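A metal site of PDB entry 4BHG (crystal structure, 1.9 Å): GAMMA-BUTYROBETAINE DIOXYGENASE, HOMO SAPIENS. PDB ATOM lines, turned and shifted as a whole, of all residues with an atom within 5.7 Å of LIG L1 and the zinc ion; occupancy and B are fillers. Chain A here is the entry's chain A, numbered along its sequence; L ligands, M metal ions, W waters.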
ATOM      1  N   TRP A 181      10.509  21.847 -18.780  1.00  0.00           N
ATOM      2  CA  TRP A 181       9.143  22.204 -18.358  1.00  0.00           C
ATOM      3  C   TRP A 181       8.156  21.759 -19.415  1.00  0.00           C
ATOM      4  O   TRP A 181       8.503  21.591 -20.595  1.00  0.00           O
ATOM      5  CB  TRP A 181       9.013  23.702 -18.078  1.00  0.00           C
ATOM      6  CG  TRP A 181       9.995  24.567 -18.792  1.00  0.00           C
ATOM      7  CD1 TRP A 181      11.203  25.011 -18.310  1.00  0.00           C
ATOM      8  CD2 TRP A 181       9.880  25.113 -20.121  1.00  0.00           C
ATOM      9  NE1 TRP A 181      11.842  25.762 -19.254  1.00  0.00           N
ATOM     10  CE2 TRP A 181      11.057  25.837 -20.370  1.00  0.00           C
ATOM     11  CE3 TRP A 181       8.912  25.032 -21.116  1.00  0.00           C
ATOM     12  CZ2 TRP A 181      11.281  26.507 -21.564  1.00  0.00           C
ATOM     13  CZ3 TRP A 181       9.131  25.700 -22.302  1.00  0.00           C
ATOM     14  CH2 TRP A 181      10.331  26.415 -22.528  1.00  0.00           C
ATOM     15  N   VAL A 183       4.732  22.285 -21.486  1.00  0.00           N
ATOM     16  CA  VAL A 183       3.758  23.230 -21.993  1.00  0.00           C
ATOM     17  C   VAL A 183       2.493  22.441 -22.298  1.00  0.00           C
ATOM     18  O   VAL A 183       2.435  21.714 -23.285  1.00  0.00           O
ATOM     19  CB  VAL A 183       4.237  23.981 -23.260  1.00  0.00           C
ATOM     20  CG1 VAL A 183       3.252  25.082 -23.637  1.00  0.00           C
ATOM     21  CG2 VAL A 183       5.637  24.539 -23.067  1.00  0.00           C
ATOM     22  N   ALA A 193       1.272  30.564 -20.690  1.00  0.00           N
ATOM     23  CA  ALA A 193       1.693  29.533 -21.609  1.00  0.00           C
ATOM     24  C   ALA A 193       1.085  28.159 -21.265  1.00  0.00           C
ATOM     25  O   ALA A 193       0.916  27.323 -22.163  1.00  0.00           O
ATOM     26  CB  ALA A 193       3.222  29.466 -21.646  1.00  0.00           C
ATOM     27  N   TYR A 194       0.716  27.947 -20.001  1.00  0.00           N
ATOM     28  CA  TYR A 194       0.161  26.670 -19.527  1.00  0.00           C
ATOM     29  C   TYR A 194      -1.390  26.699 -19.545  1.00  0.00           C
ATOM     30  O   TYR A 194      -2.042  26.231 -18.609  1.00  0.00           O
ATOM     31  CB  TYR A 194       0.656  26.382 -18.117  1.00  0.00           C
ATOM     32  CG  TYR A 194       2.182  26.266 -18.002  1.00  0.00           C
ATOM     33  CD1 TYR A 194       2.962  25.825 -19.098  1.00  0.00           C
ATOM     34  CD2 TYR A 194       2.815  26.514 -16.801  1.00  0.00           C
ATOM     35  CE1 TYR A 194       4.336  25.694 -18.979  1.00  0.00           C
ATOM     36  CE2 TYR A 194       4.218  26.397 -16.674  1.00  0.00           C
ATOM     37  CZ  TYR A 194       4.958  25.948 -17.760  1.00  0.00           C
ATOM     38  OH  TYR A 194       6.324  25.819 -17.668  1.00  0.00           O
ATOM     39  N   LEU A 199      -0.836  32.723 -27.678  1.00  0.00           N
ATOM     40  CA  LEU A 199       0.283  33.524 -27.244  1.00  0.00           C
ATOM     41  C   LEU A 199       0.640  34.408 -28.424  1.00  0.00           C
ATOM     42  O   LEU A 199       0.982  33.893 -29.515  1.00  0.00           O
ATOM     43  CB  LEU A 199       1.483  32.630 -26.854  1.00  0.00           C
ATOM     44  CG  LEU A 199       1.219  31.615 -25.730  1.00  0.00           C
ATOM     45  CD1 LEU A 199       2.475  30.793 -25.447  1.00  0.00           C
ATOM     46  CD2 LEU A 199       0.728  32.312 -24.476  1.00  0.00           C
ATOM     47  N   HIS A 202       6.114  37.012 -28.590  1.00  0.00           N
ATOM     48  CA  HIS A 202       6.880  37.395 -27.402  1.00  0.00           C
ATOM     49  C   HIS A 202       8.259  36.763 -27.442  1.00  0.00           C
ATOM     50  O   HIS A 202       8.505  35.842 -28.239  1.00  0.00           O
ATOM     51  CB  HIS A 202       6.146  36.940 -26.149  1.00  0.00           C
ATOM     52  CG  HIS A 202       5.977  35.454 -26.059  1.00  0.00           C
ATOM     53  ND1 HIS A 202       5.083  34.758 -26.835  1.00  0.00           N
ATOM     54  CD2 HIS A 202       6.627  34.532 -25.321  1.00  0.00           C
ATOM     55  CE1 HIS A 202       5.175  33.469 -26.569  1.00  0.00           C
ATOM     56  NE2 HIS A 202       6.123  33.312 -25.658  1.00  0.00           N
ATOM     57  N   THR A 203       9.149  37.276 -26.589  1.00  0.00           N
ATOM     58  CA  THR A 203      10.337  36.573 -26.191  1.00  0.00           C
ATOM     59  C   THR A 203      10.098  35.971 -24.804  1.00  0.00           C
ATOM     60  O   THR A 203       9.269  36.460 -24.029  1.00  0.00           O
ATOM     61  CB  THR A 203      11.582  37.509 -26.136  1.00  0.00           C
ATOM     62  OG1 THR A 203      11.371  38.571 -25.185  1.00  0.00           O
ATOM     63  CG2 THR A 203      11.888  38.108 -27.497  1.00  0.00           C
ATOM     64  N   ASP A 204      10.787  34.879 -24.499  1.00  0.00           N
ATOM     65  CA  ASP A 204      10.599  34.207 -23.227  1.00  0.00           C
ATOM     66  C   ASP A 204      11.449  34.882 -22.154  1.00  0.00           C
ATOM     67  O   ASP A 204      12.619  35.171 -22.355  1.00  0.00           O
ATOM     68  CB  ASP A 204      10.982  32.737 -23.289  1.00  0.00           C
ATOM     69  CG  ASP A 204       9.784  31.834 -23.568  1.00  0.00           C
ATOM     70  OD1 ASP A 204       8.927  32.265 -24.325  1.00  0.00           O
ATOM     71  OD2 ASP A 204       9.727  30.721 -23.000  1.00  0.00           O
ATOM     72  N   GLN A 215      16.165  28.831 -26.892  1.00  0.00           N
ATOM     73  CA  GLN A 215      15.061  28.062 -26.402  1.00  0.00           C
ATOM     74  C   GLN A 215      14.909  26.804 -27.236  1.00  0.00           C
ATOM     75  O   GLN A 215      15.082  26.835 -28.450  1.00  0.00           O
ATOM     76  CB  GLN A 215      13.781  28.905 -26.450  1.00  0.00           C
ATOM     77  CG  GLN A 215      12.550  28.236 -25.859  1.00  0.00           C
ATOM     78  CD  GLN A 215      11.368  29.185 -25.714  1.00  0.00           C
ATOM     79  OE1 GLN A 215      10.187  28.770 -25.672  1.00  0.00           O
ATOM     80  NE2 GLN A 215      11.666  30.470 -25.632  1.00  0.00           N
ATOM     81  N   LEU A 217      12.047  23.684 -27.964  1.00  0.00           N
ATOM     82  CA  LEU A 217      10.700  23.193 -27.764  1.00  0.00           C
ATOM     83  C   LEU A 217      10.499  21.898 -28.528  1.00  0.00           C
ATOM     84  O   LEU A 217      10.663  21.878 -29.758  1.00  0.00           O
ATOM     85  CB  LEU A 217       9.651  24.204 -28.254  1.00  0.00           C
ATOM     86  CG  LEU A 217       9.406  25.481 -27.442  1.00  0.00           C
ATOM     87  CD1 LEU A 217       8.366  26.354 -28.141  1.00  0.00           C
ATOM     88  CD2 LEU A 217       8.945  25.106 -26.052  1.00  0.00           C
ATOM     89  N   GLY A 227      -3.113  25.587 -32.225  1.00  0.00           N
ATOM     90  CA  GLY A 227      -1.744  25.398 -31.689  1.00  0.00           C
ATOM     91  C   GLY A 227      -0.613  25.454 -32.696  1.00  0.00           C
ATOM     92  O   GLY A 227       0.492  24.975 -32.415  1.00  0.00           O
ATOM     93  N   ASP A 228      -0.871  26.031 -33.866  1.00  0.00           N
ATOM     94  CA  ASP A 228       0.179  26.342 -34.819  1.00  0.00           C
ATOM     95  C   ASP A 228       1.189  27.320 -34.211  1.00  0.00           C
ATOM     96  O   ASP A 228       0.841  28.147 -33.363  1.00  0.00           O
ATOM     97  CB  ASP A 228      -0.375  27.022 -36.077  1.00  0.00           C
ATOM     98  CG  ASP A 228      -1.482  26.235 -36.712  1.00  0.00           C
ATOM     99  OD1 ASP A 228      -2.553  26.170 -36.083  1.00  0.00           O
ATOM    100  OD2 ASP A 228      -1.252  25.693 -37.825  1.00  0.00           O
ATOM    101  N   SER A 229       2.415  27.255 -34.723  1.00  0.00           N
ATOM    102  CA  SER A 229       3.503  28.102 -34.285  1.00  0.00           C
ATOM    103  C   SER A 229       3.682  29.269 -35.251  1.00  0.00           C
ATOM    104  O   SER A 229       3.367  29.199 -36.469  1.00  0.00           O
ATOM    105  CB  SER A 229       4.805  27.300 -34.204  1.00  0.00           C
ATOM    106  OG  SER A 229       4.702  26.243 -33.289  1.00  0.00           O
ATOM    107  N   HIS A 347       8.221  34.638 -30.863  1.00  0.00           N
ATOM    108  CA  HIS A 347       7.451  33.467 -31.211  1.00  0.00           C
ATOM    109  C   HIS A 347       6.066  33.544 -30.589  1.00  0.00           C
ATOM    110  O   HIS A 347       5.778  34.331 -29.657  1.00  0.00           O
ATOM    111  CB  HIS A 347       8.194  32.190 -30.809  1.00  0.00           C
ATOM    112  CG  HIS A 347       8.412  32.041 -29.328  1.00  0.00           C
ATOM    113  ND1 HIS A 347       9.390  32.742 -28.655  1.00  0.00           N
ATOM    114  CD2 HIS A 347       7.800  31.276 -28.407  1.00  0.00           C
ATOM    115  CE1 HIS A 347       9.357  32.430 -27.373  1.00  0.00           C
ATOM    116  NE2 HIS A 347       8.381  31.553 -27.182  1.00  0.00           N
ATOM    117  N   GLY A 348       5.185  32.735 -31.148  1.00  0.00           N
ATOM    118  CA  GLY A 348       3.816  32.701 -30.691  1.00  0.00           C
ATOM    119  C   GLY A 348       3.170  31.382 -30.988  1.00  0.00           C
ATOM    120  O   GLY A 348       3.752  30.510 -31.632  1.00  0.00           O
ATOM    121  N   ARG A 349       1.935  31.281 -30.551  1.00  0.00           N
ATOM    122  CA  ARG A 349       1.147  30.100 -30.748  1.00  0.00           C
ATOM    123  C   ARG A 349      -0.325  30.463 -30.899  1.00  0.00           C
ATOM    124  O   ARG A 349      -0.868  31.312 -30.179  1.00  0.00           O
ATOM    125  CB  ARG A 349       1.313  29.180 -29.560  1.00  0.00           C
ATOM    126  CG  ARG A 349       0.168  28.261 -29.252  1.00  0.00           C
ATOM    127  CD  ARG A 349       0.333  27.667 -27.881  1.00  0.00           C
ATOM    128  NE  ARG A 349      -0.442  28.300 -26.847  1.00  0.00           N
ATOM    129  CZ  ARG A 349      -0.221  28.103 -25.561  1.00  0.00           C
ATOM    130  NH1 ARG A 349       0.791  27.341 -25.170  1.00  0.00           N
ATOM    131  NH2 ARG A 349      -0.984  28.691 -24.658  1.00  0.00           N
ATOM    132  N   ARG A 360      -2.310  18.279 -26.109  1.00  0.00           N
ATOM    133  CA  ARG A 360      -1.161  19.005 -26.606  1.00  0.00           C
ATOM    134  C   ARG A 360      -0.140  19.121 -25.469  1.00  0.00           C
ATOM    135  O   ARG A 360      -0.497  19.487 -24.347  1.00  0.00           O
ATOM    136  CB  ARG A 360      -1.553  20.410 -27.076  1.00  0.00           C
ATOM    137  CG  ARG A 360      -0.452  21.112 -27.885  1.00  0.00           C
ATOM    138  CD  ARG A 360      -0.915  22.489 -28.307  1.00  0.00           C
ATOM    139  NE  ARG A 360       0.010  23.143 -29.226  1.00  0.00           N
ATOM    140  CZ  ARG A 360       1.009  23.966 -28.889  1.00  0.00           C
ATOM    141  NH1 ARG A 360       1.308  24.234 -27.639  1.00  0.00           N
ATOM    142  NH2 ARG A 360       1.734  24.519 -29.847  1.00  0.00           N
ATOM    143  N   LEU A 362       4.167  20.052 -25.180  1.00  0.00           N
ATOM    144  CA  LEU A 362       5.551  20.288 -25.598  1.00  0.00           C
ATOM    145  C   LEU A 362       6.417  20.212 -24.343  1.00  0.00           C
ATOM    146  O   LEU A 362       5.980  20.621 -23.269  1.00  0.00           O
ATOM    147  CB  LEU A 362       5.723  21.660 -26.210  1.00  0.00           C
ATOM    148  CG  LEU A 362       4.713  22.214 -27.204  1.00  0.00           C
ATOM    149  CD1 LEU A 362       5.142  23.625 -27.605  1.00  0.00           C
ATOM    150  CD2 LEU A 362       4.626  21.300 -28.386  1.00  0.00           C
ATOM    151  N   TYR A 366      15.861  25.872 -21.826  1.00  0.00           N
ATOM    152  CA  TYR A 366      16.640  27.025 -22.224  1.00  0.00           C
ATOM    153  C   TYR A 366      18.123  26.696 -22.177  1.00  0.00           C
ATOM    154  O   TYR A 366      18.555  25.810 -21.450  1.00  0.00           O
ATOM    155  CB  TYR A 366      16.389  28.180 -21.241  1.00  0.00           C
ATOM    156  CG  TYR A 366      14.943  28.668 -21.200  1.00  0.00           C
ATOM    157  CD1 TYR A 366      14.316  29.131 -22.357  1.00  0.00           C
ATOM    158  CD2 TYR A 366      14.256  28.736 -19.999  1.00  0.00           C
ATOM    159  CE1 TYR A 366      13.002  29.590 -22.316  1.00  0.00           C
ATOM    160  CE2 TYR A 366      12.973  29.240 -19.943  1.00  0.00           C
ATOM    161  CZ  TYR A 366      12.357  29.675 -21.111  1.00  0.00           C
ATOM    162  OH  TYR A 366      11.052  30.142 -21.029  1.00  0.00           O
HETATM  163  C1  LIG L   1       5.976  29.337 -24.340  1.00  0.00           C
HETATM  164  C2  LIG L   1       5.601  29.279 -25.754  1.00  0.00           C
HETATM  165  C3  LIG L   1       4.771  27.917 -27.598  1.00  0.00           C
HETATM  166  C4  LIG L   1       3.703  26.870 -27.857  1.00  0.00           C
HETATM  167  O1  LIG L   1       5.599  28.361 -23.645  1.00  0.00           O
HETATM  168  O2  LIG L   1       6.694  30.329 -23.930  1.00  0.00           O
HETATM  169  O3  LIG L   1       5.919  30.208 -26.480  1.00  0.00           O
HETATM  170  O4  LIG L   1       3.529  26.523 -29.029  1.00  0.00           O
HETATM  171  N1  LIG L   1       4.982  28.182 -26.177  1.00  0.00           N
HETATM  172  O5  LIG L   1       3.020  26.427 -26.910  1.00  0.00           O
HETATM  173  C1  LG2 L   2       7.819  33.785 -19.657  1.00  0.00           C
HETATM  174  N1  LG2 L   2       7.835  30.528 -20.153  1.00  0.00           N
HETATM  175  O1  LG2 L   2       6.775  33.588 -18.992  1.00  0.00           O
HETATM  176  C2  LG2 L   2       8.902  32.738 -19.715  1.00  0.00           C
HETATM  177  N2  LG2 L   2       7.460  29.182 -19.894  1.00  0.00           N
HETATM  178  O2  LG2 L   2       8.046  34.855 -20.231  1.00  0.00           O
HETATM  179  C3  LG2 L   2       8.521  31.359 -19.164  1.00  0.00           C
HETATM  180  C4  LG2 L   2       6.950  28.550 -21.117  1.00  0.00           C
HETATM  181  C5  LG2 L   2       6.393  29.095 -18.870  1.00  0.00           C
HETATM  182  C6  LG2 L   2       8.626  28.322 -19.669  1.00  0.00           C
HETATM  183  C7  LG2 L   2       9.289  28.515 -18.392  1.00  0.00           C
HETATM  184 ZN    ZN M   1       7.343  31.454 -25.374  1.00  0.00          ZN
HETATM  185  O   HOH W   1       4.993  27.704 -31.040  1.00  0.00           O
HETATM  186  O   HOH W   2       6.275  32.357 -21.977  1.00  0.00           O
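The guanidinium group (NH2) of Arg 360 lies within salt-bridge range of an oxygen (O4) of LIG L1, 2.8 Å away. O5 of LIG L1 lies within salt-bridge range of NH1 of Arg 349 (3.0 Å). A nitrogen (N1) of LG2 L2 is in hydrogen-bond range of the side-chain carboxylate (OD2) of Asp 204 (3.4 Å). N1 of LG2 L2 lies close to OH of Tyr 366.
O2 of LIG L1 binds the zinc ion, at 1.9 Å. OD1 of Asp 204 binds the zinc ion. A ring nitrogen (NE2) of His 347 binds the zinc ion (2.1 Å). An oxygen (O3) of LIG L1 is bound to the zinc ion (2.2 Å). A ring nitrogen (NE2) of His 202 binds the zinc ion (2.2 Å). The zinc ion has five donor atoms within binding distance.
Val 183 touches LIG L1. Ala 193 touches LIG L1. Leu 199 touches LIG L1 (CD1 to C2, 3.5 Å). Leu 217 touches LIG L1 (CD1 to C3, 3.96 Å). CD1 of Leu 362 touches C4 of LIG L1, 3.6 Å away.
Gln 215 touches the zinc ion. The nearest printed residue that does not touch the zinc ion is Leu 199 (4.9 Å).
Water W1 lies within hydrogen-bond range of OG of Ser 229, O4 of LIG L1 and O of Gly 348.
NE2 of Gln 215 sits close to OD2 of Asp 204, 3.3 Å away. The side-chain carboxylate (OD2) of Asp 204 sits at hydrogen-bond distance from the side-chain hydroxyl (OH) of Tyr 366, 2.4 Å away. NH2 of Arg 360 is in hydrogen-bond range of O of Gly 227 (2.9 Å). The guanidinium group (NH1) of Arg 349 lies within hydrogen-bond range of the backbone carbonyl oxygen (O) of Ala 193. O of Arg 349 sits at hydrogen-bond distance from N of Leu 199, at 2.9 Å. The backbone NH of Val 183 is in hydrogen-bond range of the backbone carbonyl oxygen of Leu 362.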
